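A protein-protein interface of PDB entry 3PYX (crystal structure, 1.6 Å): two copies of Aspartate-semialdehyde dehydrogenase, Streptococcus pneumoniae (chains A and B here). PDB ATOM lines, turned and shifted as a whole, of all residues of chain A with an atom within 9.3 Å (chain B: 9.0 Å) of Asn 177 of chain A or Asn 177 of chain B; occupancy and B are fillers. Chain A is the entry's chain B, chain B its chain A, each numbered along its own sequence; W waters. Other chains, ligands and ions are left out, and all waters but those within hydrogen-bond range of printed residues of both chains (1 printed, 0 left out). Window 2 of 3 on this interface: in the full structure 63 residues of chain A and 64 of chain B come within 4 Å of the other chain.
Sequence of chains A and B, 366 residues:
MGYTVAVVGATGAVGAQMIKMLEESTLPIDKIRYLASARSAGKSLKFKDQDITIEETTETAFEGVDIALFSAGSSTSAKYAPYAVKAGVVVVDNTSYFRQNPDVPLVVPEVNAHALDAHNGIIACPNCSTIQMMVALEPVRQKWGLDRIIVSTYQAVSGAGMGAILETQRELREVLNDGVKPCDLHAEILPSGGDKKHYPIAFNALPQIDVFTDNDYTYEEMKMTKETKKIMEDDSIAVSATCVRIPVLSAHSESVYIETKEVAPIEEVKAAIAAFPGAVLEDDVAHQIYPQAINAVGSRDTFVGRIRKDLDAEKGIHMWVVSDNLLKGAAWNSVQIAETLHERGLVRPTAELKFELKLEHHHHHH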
ATOM      1  N   GLN A 169       3.304 -17.739  -3.642  1.00  0.00           N
ATOM      2  CA  GLN A 169       4.555 -18.494  -3.604  1.00  0.00           C
ATOM      3  C   GLN A 169       5.284 -18.265  -2.285  1.00  0.00           C
ATOM      4  O   GLN A 169       5.786 -19.210  -1.697  1.00  0.00           O
ATOM      5  CB  GLN A 169       5.438 -18.118  -4.789  1.00  0.00           C
ATOM      6  CG  GLN A 169       4.868 -18.608  -6.119  1.00  0.00           C
ATOM      7  CD  GLN A 169       5.710 -18.121  -7.284  1.00  0.00           C
ATOM      8  OE1 GLN A 169       6.071 -16.951  -7.342  1.00  0.00           O
ATOM      9  NE2 GLN A 169       6.047 -19.020  -8.193  1.00  0.00           N
ATOM     10  N   ARG A 170       5.319 -17.015  -1.846  1.00  0.00           N
ATOM     11  CA  ARG A 170       5.992 -16.655  -0.585  1.00  0.00           C
ATOM     12  C   ARG A 170       5.329 -17.363   0.584  1.00  0.00           C
ATOM     13  O   ARG A 170       6.008 -17.987   1.394  1.00  0.00           O
ATOM     14  CB  ARG A 170       5.927 -15.149  -0.358  1.00  0.00           C
ATOM     15  CG  ARG A 170       6.463 -14.734   1.033  1.00  0.00           C
ATOM     16  CD  ARG A 170       6.293 -13.262   1.301  1.00  0.00           C
ATOM     17  NE  ARG A 170       4.908 -12.764   1.295  1.00  0.00           N
ATOM     18  CZ  ARG A 170       3.990 -12.948   2.248  1.00  0.00           C
ATOM     19  NH1 ARG A 170       2.796 -12.387   2.119  1.00  0.00           N
ATOM     20  NH2 ARG A 170       4.237 -13.682   3.319  1.00  0.00           N
ATOM     21  N   GLU A 171       3.998 -17.268   0.652  1.00  0.00           N
ATOM     22  CA  GLU A 171       3.212 -17.904   1.735  1.00  0.00           C
ATOM     23  C   GLU A 171       3.469 -19.392   1.808  1.00  0.00           C
ATOM     24  O   GLU A 171       3.701 -19.926   2.899  1.00  0.00           O
ATOM     25  CB  GLU A 171       1.705 -17.630   1.560  1.00  0.00           C
ATOM     26  CG  GLU A 171       1.312 -16.231   1.979  1.00  0.00           C
ATOM     27  CD  GLU A 171      -0.151 -15.892   1.764  1.00  0.00           C
ATOM     28  OE1 GLU A 171      -0.974 -16.805   1.514  1.00  0.00           O
ATOM     29  OE2 GLU A 171      -0.511 -14.703   1.827  1.00  0.00           O
ATOM     30  N   LEU A 172       3.397 -20.077   0.661  1.00  0.00           N
ATOM     31  CA  LEU A 172       3.638 -21.515   0.620  1.00  0.00           C
ATOM     32  C   LEU A 172       5.037 -21.896   1.088  1.00  0.00           C
ATOM     33  O   LEU A 172       5.208 -22.900   1.796  1.00  0.00           O
ATOM     34  CB  LEU A 172       3.363 -22.082  -0.773  1.00  0.00           C
ATOM     35  CG  LEU A 172       1.873 -22.102  -1.126  1.00  0.00           C
ATOM     36  CD1 LEU A 172       1.671 -22.167  -2.641  1.00  0.00           C
ATOM     37  CD2 LEU A 172       1.179 -23.257  -0.398  1.00  0.00           C
ATOM     38  N   ARG A 173       6.031 -21.090   0.703  1.00  0.00           N
ATOM     39  CA  ARG A 173       7.413 -21.344   1.115  1.00  0.00           C
ATOM     40  C   ARG A 173       7.557 -21.164   2.635  1.00  0.00           C
ATOM     41  O   ARG A 173       8.240 -21.952   3.298  1.00  0.00           O
ATOM     42  CB  ARG A 173       8.382 -20.437   0.353  1.00  0.00           C
ATOM     43  CG  ARG A 173       8.636 -20.912  -1.064  1.00  0.00           C
ATOM     44  CD  ARG A 173       9.495 -19.925  -1.850  1.00  0.00           C
ATOM     45  NE  ARG A 173       9.831 -20.473  -3.167  1.00  0.00           N
ATOM     46  CZ  ARG A 173       9.597 -19.876  -4.332  1.00  0.00           C
ATOM     47  NH1 ARG A 173       9.040 -18.672  -4.387  1.00  0.00           N
ATOM     48  NH2 ARG A 173       9.947 -20.492  -5.449  1.00  0.00           N
ATOM     49  N   GLU A 174       6.884 -20.164   3.185  1.00  0.00           N
ATOM     50  CA  GLU A 174       6.954 -19.931   4.639  1.00  0.00           C
ATOM     51  C   GLU A 174       6.373 -21.118   5.391  1.00  0.00           C
ATOM     52  O   GLU A 174       6.944 -21.587   6.372  1.00  0.00           O
ATOM     53  CB  GLU A 174       6.264 -18.622   5.029  1.00  0.00           C
ATOM     54  CG  GLU A 174       7.006 -17.377   4.525  1.00  0.00           C
ATOM     55  CD  GLU A 174       6.308 -16.069   4.843  1.00  0.00           C
ATOM     56  OE1 GLU A 174       5.351 -16.064   5.630  1.00  0.00           O
ATOM     57  OE2 GLU A 174       6.729 -15.015   4.307  1.00  0.00           O
ATOM     58  N   VAL A 175       5.247 -21.634   4.918  1.00  0.00           N
ATOM     59  CA  VAL A 175       4.665 -22.832   5.541  1.00  0.00           C
ATOM     60  C   VAL A 175       5.537 -24.090   5.381  1.00  0.00           C
ATOM     61  O   VAL A 175       5.856 -24.773   6.369  1.00  0.00           O
ATOM     62  CB  VAL A 175       3.230 -23.108   5.005  1.00  0.00           C
ATOM     63  CG1 VAL A 175       2.654 -24.349   5.656  1.00  0.00           C
ATOM     64  CG2 VAL A 175       2.327 -21.924   5.269  1.00  0.00           C
ATOM     65  N   LEU A 176       5.964 -24.369   4.155  1.00  0.00           N
ATOM     66  CA  LEU A 176       6.568 -25.650   3.824  1.00  0.00           C
ATOM     67  C   LEU A 176       8.045 -25.755   4.155  1.00  0.00           C
ATOM     68  O   LEU A 176       8.563 -26.866   4.364  1.00  0.00           O
ATOM     69  CB  LEU A 176       6.385 -25.925   2.333  1.00  0.00           C
ATOM     70  CG  LEU A 176       4.949 -26.256   1.942  1.00  0.00           C
ATOM     71  CD1 LEU A 176       4.815 -26.106   0.441  1.00  0.00           C
ATOM     72  CD2 LEU A 176       4.584 -27.669   2.395  1.00  0.00           C
ATOM     73  N   ASN A 177       8.719 -24.612   4.172  1.00  0.00           N
ATOM     74  CA  ASN A 177      10.162 -24.585   4.416  1.00  0.00           C
ATOM     75  C   ASN A 177      10.497 -24.052   5.798  1.00  0.00           C
ATOM     76  O   ASN A 177      11.486 -24.491   6.404  1.00  0.00           O
ATOM     77  CB  ASN A 177      10.884 -23.756   3.353  1.00  0.00           C
ATOM     78  CG  ASN A 177      10.757 -24.344   1.964  1.00  0.00           C
ATOM     79  OD1 ASN A 177      10.566 -25.558   1.788  1.00  0.00           O
ATOM     80  ND2 ASN A 177      10.895 -23.489   0.960  1.00  0.00           N
ATOM     81  N   ASP A 178       9.692 -23.102   6.282  1.00  0.00           N
ATOM     82  CA  ASP A 178       9.941 -22.461   7.586  1.00  0.00           C
ATOM     83  C   ASP A 178       9.043 -22.959   8.735  1.00  0.00           C
ATOM     84  O   ASP A 178       9.329 -22.707   9.908  1.00  0.00           O
ATOM     85  CB  ASP A 178       9.851 -20.930   7.477  1.00  0.00           C
ATOM     86  CG  ASP A 178      10.829 -20.343   6.463  1.00  0.00           C
ATOM     87  OD1 ASP A 178      11.854 -20.992   6.157  1.00  0.00           O
ATOM     88  OD2 ASP A 178      10.571 -19.223   5.966  1.00  0.00           O
ATOM     89  N   GLY A 179       7.967 -23.668   8.412  1.00  0.00           N
ATOM     90  CA  GLY A 179       7.073 -24.200   9.444  1.00  0.00           C
ATOM     91  C   GLY A 179       6.076 -23.206  10.019  1.00  0.00           C
ATOM     92  O   GLY A 179       5.529 -23.434  11.094  1.00  0.00           O
ATOM     93  N   VAL A 180       5.845 -22.100   9.313  1.00  0.00           N
ATOM     94  CA  VAL A 180       4.828 -21.120   9.700  1.00  0.00           C
ATOM     95  C   VAL A 180       3.422 -21.733   9.592  1.00  0.00           C
ATOM     96  O   VAL A 180       3.138 -22.490   8.661  1.00  0.00           O
ATOM     97  CB  VAL A 180       4.923 -19.845   8.819  1.00  0.00           C
ATOM     98  CG1 VAL A 180       3.819 -18.855   9.149  1.00  0.00           C
ATOM     99  CG2 VAL A 180       6.285 -19.177   8.984  1.00  0.00           C
ATOM    100  N   PHE A 203      -2.901 -23.034   1.477  1.00  0.00           N
ATOM    101  CA  PHE A 203      -3.673 -24.092   2.152  1.00  0.00           C
ATOM    102  C   PHE A 203      -5.079 -23.638   2.551  1.00  0.00           C
ATOM    103  O   PHE A 203      -5.668 -24.129   3.533  1.00  0.00           O
ATOM    104  CB  PHE A 203      -2.853 -24.653   3.339  1.00  0.00           C
ATOM    105  CG  PHE A 203      -1.552 -25.266   2.907  1.00  0.00           C
ATOM    106  CD1 PHE A 203      -1.540 -26.480   2.229  1.00  0.00           C
ATOM    107  CD2 PHE A 203      -0.336 -24.589   3.108  1.00  0.00           C
ATOM    108  CE1 PHE A 203      -0.333 -27.052   1.792  1.00  0.00           C
ATOM    109  CE2 PHE A 203       0.868 -25.155   2.673  1.00  0.00           C
ATOM    110  CZ  PHE A 203       0.870 -26.397   2.034  1.00  0.00           C
ATOM    111  N   GLN B 169       2.734 -32.289   0.526  1.00  0.00           N
ATOM    112  CA  GLN B 169       3.819 -31.437   1.005  1.00  0.00           C
ATOM    113  C   GLN B 169       5.089 -31.622   0.169  1.00  0.00           C
ATOM    114  O   GLN B 169       5.740 -30.648  -0.172  1.00  0.00           O
ATOM    115  CB  GLN B 169       4.101 -31.701   2.492  1.00  0.00           C
ATOM    116  CG  GLN B 169       3.006 -31.178   3.416  1.00  0.00           C
ATOM    117  CD  GLN B 169       3.189 -31.616   4.867  1.00  0.00           C
ATOM    118  OE1 GLN B 169       3.478 -32.773   5.147  1.00  0.00           O
ATOM    119  NE2 GLN B 169       2.996 -30.692   5.789  1.00  0.00           N
ATOM    120  N   ARG B 170       5.427 -32.865  -0.143  1.00  0.00           N
ATOM    121  CA  ARG B 170       6.595 -33.169  -0.966  1.00  0.00           C
ATOM    122  C   ARG B 170       6.457 -32.553  -2.367  1.00  0.00           C
ATOM    123  O   ARG B 170       7.406 -31.931  -2.883  1.00  0.00           O
ATOM    124  CB  ARG B 170       6.772 -34.674  -1.081  1.00  0.00           C
ATOM    125  CG  ARG B 170       7.870 -35.110  -2.059  1.00  0.00           C
ATOM    126  CD  ARG B 170       7.366 -36.310  -2.810  1.00  0.00           C
ATOM    127  NE  ARG B 170       7.081 -36.005  -4.179  1.00  0.00           N
ATOM    128  CZ  ARG B 170       6.217 -36.650  -4.947  1.00  0.00           C
ATOM    129  NH1 ARG B 170       5.474 -37.657  -4.490  1.00  0.00           N
ATOM    130  NH2 ARG B 170       6.094 -36.252  -6.194  1.00  0.00           N
ATOM    131  N   GLU B 171       5.281 -32.720  -2.975  1.00  0.00           N
ATOM    132  CA  GLU B 171       5.042 -32.187  -4.330  1.00  0.00           C
ATOM    133  C   GLU B 171       5.213 -30.682  -4.360  1.00  0.00           C
ATOM    134  O   GLU B 171       5.872 -30.154  -5.255  1.00  0.00           O
ATOM    135  CB  GLU B 171       3.655 -32.578  -4.869  1.00  0.00           C
ATOM    136  CG  GLU B 171       3.519 -34.036  -5.260  1.00  0.00           C
ATOM    137  CD  GLU B 171       2.132 -34.404  -5.734  1.00  0.00           C
ATOM    138  OE1 GLU B 171       1.292 -33.497  -5.929  1.00  0.00           O
ATOM    139  OE2 GLU B 171       1.872 -35.620  -5.868  1.00  0.00           O
ATOM    140  N   LEU B 172       4.613 -29.991  -3.388  1.00  0.00           N
ATOM    141  CA  LEU B 172       4.698 -28.535  -3.313  1.00  0.00           C
ATOM    142  C   LEU B 172       6.146 -28.067  -3.141  1.00  0.00           C
ATOM    143  O   LEU B 172       6.574 -27.094  -3.762  1.00  0.00           O
ATOM    144  CB  LEU B 172       3.821 -27.982  -2.193  1.00  0.00           C
ATOM    145  CG  LEU B 172       2.319 -27.964  -2.519  1.00  0.00           C
ATOM    146  CD1 LEU B 172       1.524 -27.747  -1.226  1.00  0.00           C
ATOM    147  CD2 LEU B 172       1.988 -26.911  -3.594  1.00  0.00           C
ATOM    148  N   ARG B 173       6.894 -28.789  -2.315  1.00  0.00           N
ATOM    149  CA  ARG B 173       8.323 -28.494  -2.146  1.00  0.00           C
ATOM    150  C   ARG B 173       9.106 -28.680  -3.435  1.00  0.00           C
ATOM    151  O   ARG B 173       9.959 -27.848  -3.757  1.00  0.00           O
ATOM    152  CB  ARG B 173       8.931 -29.332  -1.019  1.00  0.00           C
ATOM    153  CG  ARG B 173       8.408 -28.954   0.362  1.00  0.00           C
ATOM    154  CD  ARG B 173       9.107 -29.731   1.470  1.00  0.00           C
ATOM    155  NE  ARG B 173       8.619 -29.293   2.776  1.00  0.00           N
ATOM    156  CZ  ARG B 173       8.009 -30.074   3.668  1.00  0.00           C
ATOM    157  NH1 ARG B 173       7.806 -31.367   3.428  1.00  0.00           N
ATOM    158  NH2 ARG B 173       7.601 -29.558   4.817  1.00  0.00           N
ATOM    159  N   GLU B 174       8.819 -29.749  -4.180  1.00  0.00           N
ATOM    160  CA  GLU B 174       9.505 -29.998  -5.460  1.00  0.00           C
ATOM    161  C   GLU B 174       9.264 -28.862  -6.465  1.00  0.00           C
ATOM    162  O   GLU B 174      10.175 -28.451  -7.195  1.00  0.00           O
ATOM    163  CB  GLU B 174       9.064 -31.341  -6.066  1.00  0.00           C
ATOM    164  CG  GLU B 174       9.621 -32.583  -5.361  1.00  0.00           C
ATOM    165  CD  GLU B 174       9.549 -33.826  -6.243  1.00  0.00           C
ATOM    166  OE1 GLU B 174      10.589 -34.212  -6.817  1.00  0.00           O
ATOM    167  OE2 GLU B 174       8.459 -34.394  -6.418  1.00  0.00           O
ATOM    168  N   VAL B 175       8.033 -28.357  -6.508  1.00  0.00           N
ATOM    169  CA  VAL B 175       7.707 -27.256  -7.412  1.00  0.00           C
ATOM    170  C   VAL B 175       8.381 -25.973  -6.943  1.00  0.00           C
ATOM    171  O   VAL B 175       9.073 -25.301  -7.717  1.00  0.00           O
ATOM    172  CB  VAL B 175       6.186 -27.030  -7.495  1.00  0.00           C
ATOM    173  CG1 VAL B 175       5.876 -25.806  -8.360  1.00  0.00           C
ATOM    174  CG2 VAL B 175       5.509 -28.279  -8.033  1.00  0.00           C
ATOM    175  N   LEU B 176       8.210 -25.659  -5.663  1.00  0.00           N
ATOM    176  CA  LEU B 176       8.671 -24.382  -5.118  1.00  0.00           C
ATOM    177  C   LEU B 176      10.189 -24.309  -4.929  1.00  0.00           C
ATOM    178  O   LEU B 176      10.781 -23.232  -5.108  1.00  0.00           O
ATOM    179  CB  LEU B 176       7.944 -24.057  -3.803  1.00  0.00           C
ATOM    180  CG  LEU B 176       6.449 -23.705  -3.957  1.00  0.00           C
ATOM    181  CD1 LEU B 176       5.726 -23.870  -2.628  1.00  0.00           C
ATOM    182  CD2 LEU B 176       6.256 -22.299  -4.517  1.00  0.00           C
ATOM    183  N   ASN B 177      10.797 -25.453  -4.600  1.00  0.00           N
ATOM    184  CA  ASN B 177      12.228 -25.541  -4.267  1.00  0.00           C
ATOM    185  C   ASN B 177      13.124 -26.093  -5.374  1.00  0.00           C
ATOM    186  O   ASN B 177      14.302 -25.742  -5.433  1.00  0.00           O
ATOM    187  CB  ASN B 177      12.456 -26.344  -2.973  1.00  0.00           C
ATOM    188  CG  ASN B 177      11.729 -25.752  -1.761  1.00  0.00           C
ATOM    189  OD1 ASN B 177      11.416 -24.552  -1.719  1.00  0.00           O
ATOM    190  ND2 ASN B 177      11.440 -26.608  -0.771  1.00  0.00           N
ATOM    191  N   ASP B 178      12.587 -26.963  -6.231  1.00  0.00           N
ATOM    192  CA  ASP B 178      13.386 -27.585  -7.298  1.00  0.00           C
ATOM    193  C   ASP B 178      12.999 -27.121  -8.688  1.00  0.00           C
ATOM    194  O   ASP B 178      13.645 -27.512  -9.665  1.00  0.00           O
ATOM    195  CB  ASP B 178      13.288 -29.116  -7.265  1.00  0.00           C
ATOM    196  CG  ASP B 178      13.714 -29.710  -5.941  1.00  0.00           C
ATOM    197  OD1 ASP B 178      14.480 -29.062  -5.199  1.00  0.00           O
ATOM    198  OD2 ASP B 178      13.270 -30.838  -5.641  1.00  0.00           O
ATOM    199  N   GLY B 179      11.930 -26.329  -8.771  1.00  0.00           N
ATOM    200  CA  GLY B 179      11.447 -25.785 -10.035  1.00  0.00           C
ATOM    201  C   GLY B 179      10.801 -26.791 -10.962  1.00  0.00           C
ATOM    202  O   GLY B 179      10.755 -26.563 -12.172  1.00  0.00           O
ATOM    203  N   VAL B 180      10.310 -27.906 -10.410  1.00  0.00           N
ATOM    204  CA  VAL B 180       9.584 -28.912 -11.190  1.00  0.00           C
ATOM    205  C   VAL B 180       8.248 -28.327 -11.654  1.00  0.00           C
ATOM    206  O   VAL B 180       7.569 -27.648 -10.879  1.00  0.00           O
ATOM    207  CB  VAL B 180       9.339 -30.204 -10.366  1.00  0.00           C
ATOM    208  CG1 VAL B 180       8.583 -31.251 -11.182  1.00  0.00           C
ATOM    209  CG2 VAL B 180      10.662 -30.792  -9.872  1.00  0.00           C
ATOM    210  N   PHE B 203      -0.760 -27.379  -6.831  1.00  0.00           N
ATOM    211  CA  PHE B 203      -1.275 -26.345  -7.769  1.00  0.00           C
ATOM    212  C   PHE B 203      -2.343 -26.894  -8.729  1.00  0.00           C
ATOM    213  O   PHE B 203      -2.470 -26.441  -9.881  1.00  0.00           O
ATOM    214  CB  PHE B 203      -0.108 -25.690  -8.540  1.00  0.00           C
ATOM    215  CG  PHE B 203       0.869 -25.016  -7.643  1.00  0.00           C
ATOM    216  CD1 PHE B 203       0.532 -23.824  -7.005  1.00  0.00           C
ATOM    217  CD2 PHE B 203       2.097 -25.615  -7.361  1.00  0.00           C
ATOM    218  CE1 PHE B 203       1.452 -23.188  -6.127  1.00  0.00           C
ATOM    219  CE2 PHE B 203       3.008 -25.002  -6.481  1.00  0.00           C
ATOM    220  CZ  PHE B 203       2.680 -23.780  -5.877  1.00  0.00           C
HETATM  221  O   HOH W   1      12.154 -22.155  -2.394  1.00  0.00           O
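Among the printed residues, pairs that only touch across the chains: Leu 176 of chain A with Leu 172 of chain B (3.4 Å), Leu 172 of chain A with Leu 176 of chain B (3.5 Å), Phe 203 of chain A with Leu 172 of chain B (3.6 Å), Leu 172 of chain A with Phe 203 of chain B (3.6 Å), Leu 176 of chain A with Leu 176 of chain B (3.9 Å) and Leu 176 of chain A with Gln 169 of chain B (3.98 Å).
Of the printed residues of chain B, Arg 173 of chain A touches Leu 176. Val 175 of chain A touches none of the printed residues of chain B. Of the printed residues of chain B, Leu 176 of chain A touches Gln 169, Leu 172, Arg 173 and Leu 176. Of chain B, only Asn 177 (2.9 Å) comes within 4 Å of Asn 177 of chain A. No residue of chain B comes within 4 Å of Asp 178 of chain A. Printed residues of chain B within 4 Å of Phe 203 of chain A: Leu 172 (3.6 Å). Printed residues of chain A within 4 Å of Gln 169 of chain B: Leu 176. Printed residues of chain A within 4 Å of Leu 176 of chain B: Leu 172, Arg 173 and Leu 176. Of chain A, only Asn 177 comes within 4 Å of Asn 177 of chain B. No residue of chain A comes within 4 Å of Asp 178 of chain B.
The guanidinium group (NH2) of Arg 173 of chain B lies within hydrogen-bond range of the backbone carbonyl oxygen (O) of Leu 176 of chain A. O of Leu 176 of chain B is in hydrogen-bond range of NH2 of Arg 173 of chain A, at 2.9 Å. OD1 of Asn 177 of chain A lies within hydrogen-bond range of ND2 of Asn 177 of chain B (2.9 Å).
Hydrophobic or aromatic side chains of chain A within 4 Å of the printed part of chain B: Leu 172, Leu 176 and Phe 203. Of the 13 printed residues of chain B, 6 touch a printed residue of chain A. Among the printed residues, no Asp or Glu carboxylate lies within 4 Å of a Lys or Arg side-chain nitrogen of the other chain.
Water W1 lies within hydrogen-bond range of OD1 of Asn 177 of chain B (2.6 Å), NE of Arg 173 of chain A (3.0 Å) and O of Leu 176 of chain B (3.2 Å).
Leu 172 of chain A touches Leu 176 of chain B, and with the chains exchanged Leu 176 of chain A touches Leu 172 of chain B. Leu 172 of chain A touches Phe 203 of chain B, and with the chains exchanged Phe 203 of chain A touches Leu 172 of chain B. Arg 173 of chain A touches Leu 176 of chain B, and with the chains exchanged Leu 176 of chain A touches Arg 173 of chain B. Leu 176 of chain B touches its own counterpart, Leu 176 of chain A. 13 positions are printed for both chains. Of the 9 pairs that touch across the chains among the printed residues, 8 have their exchanged pair printed and touching as well.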
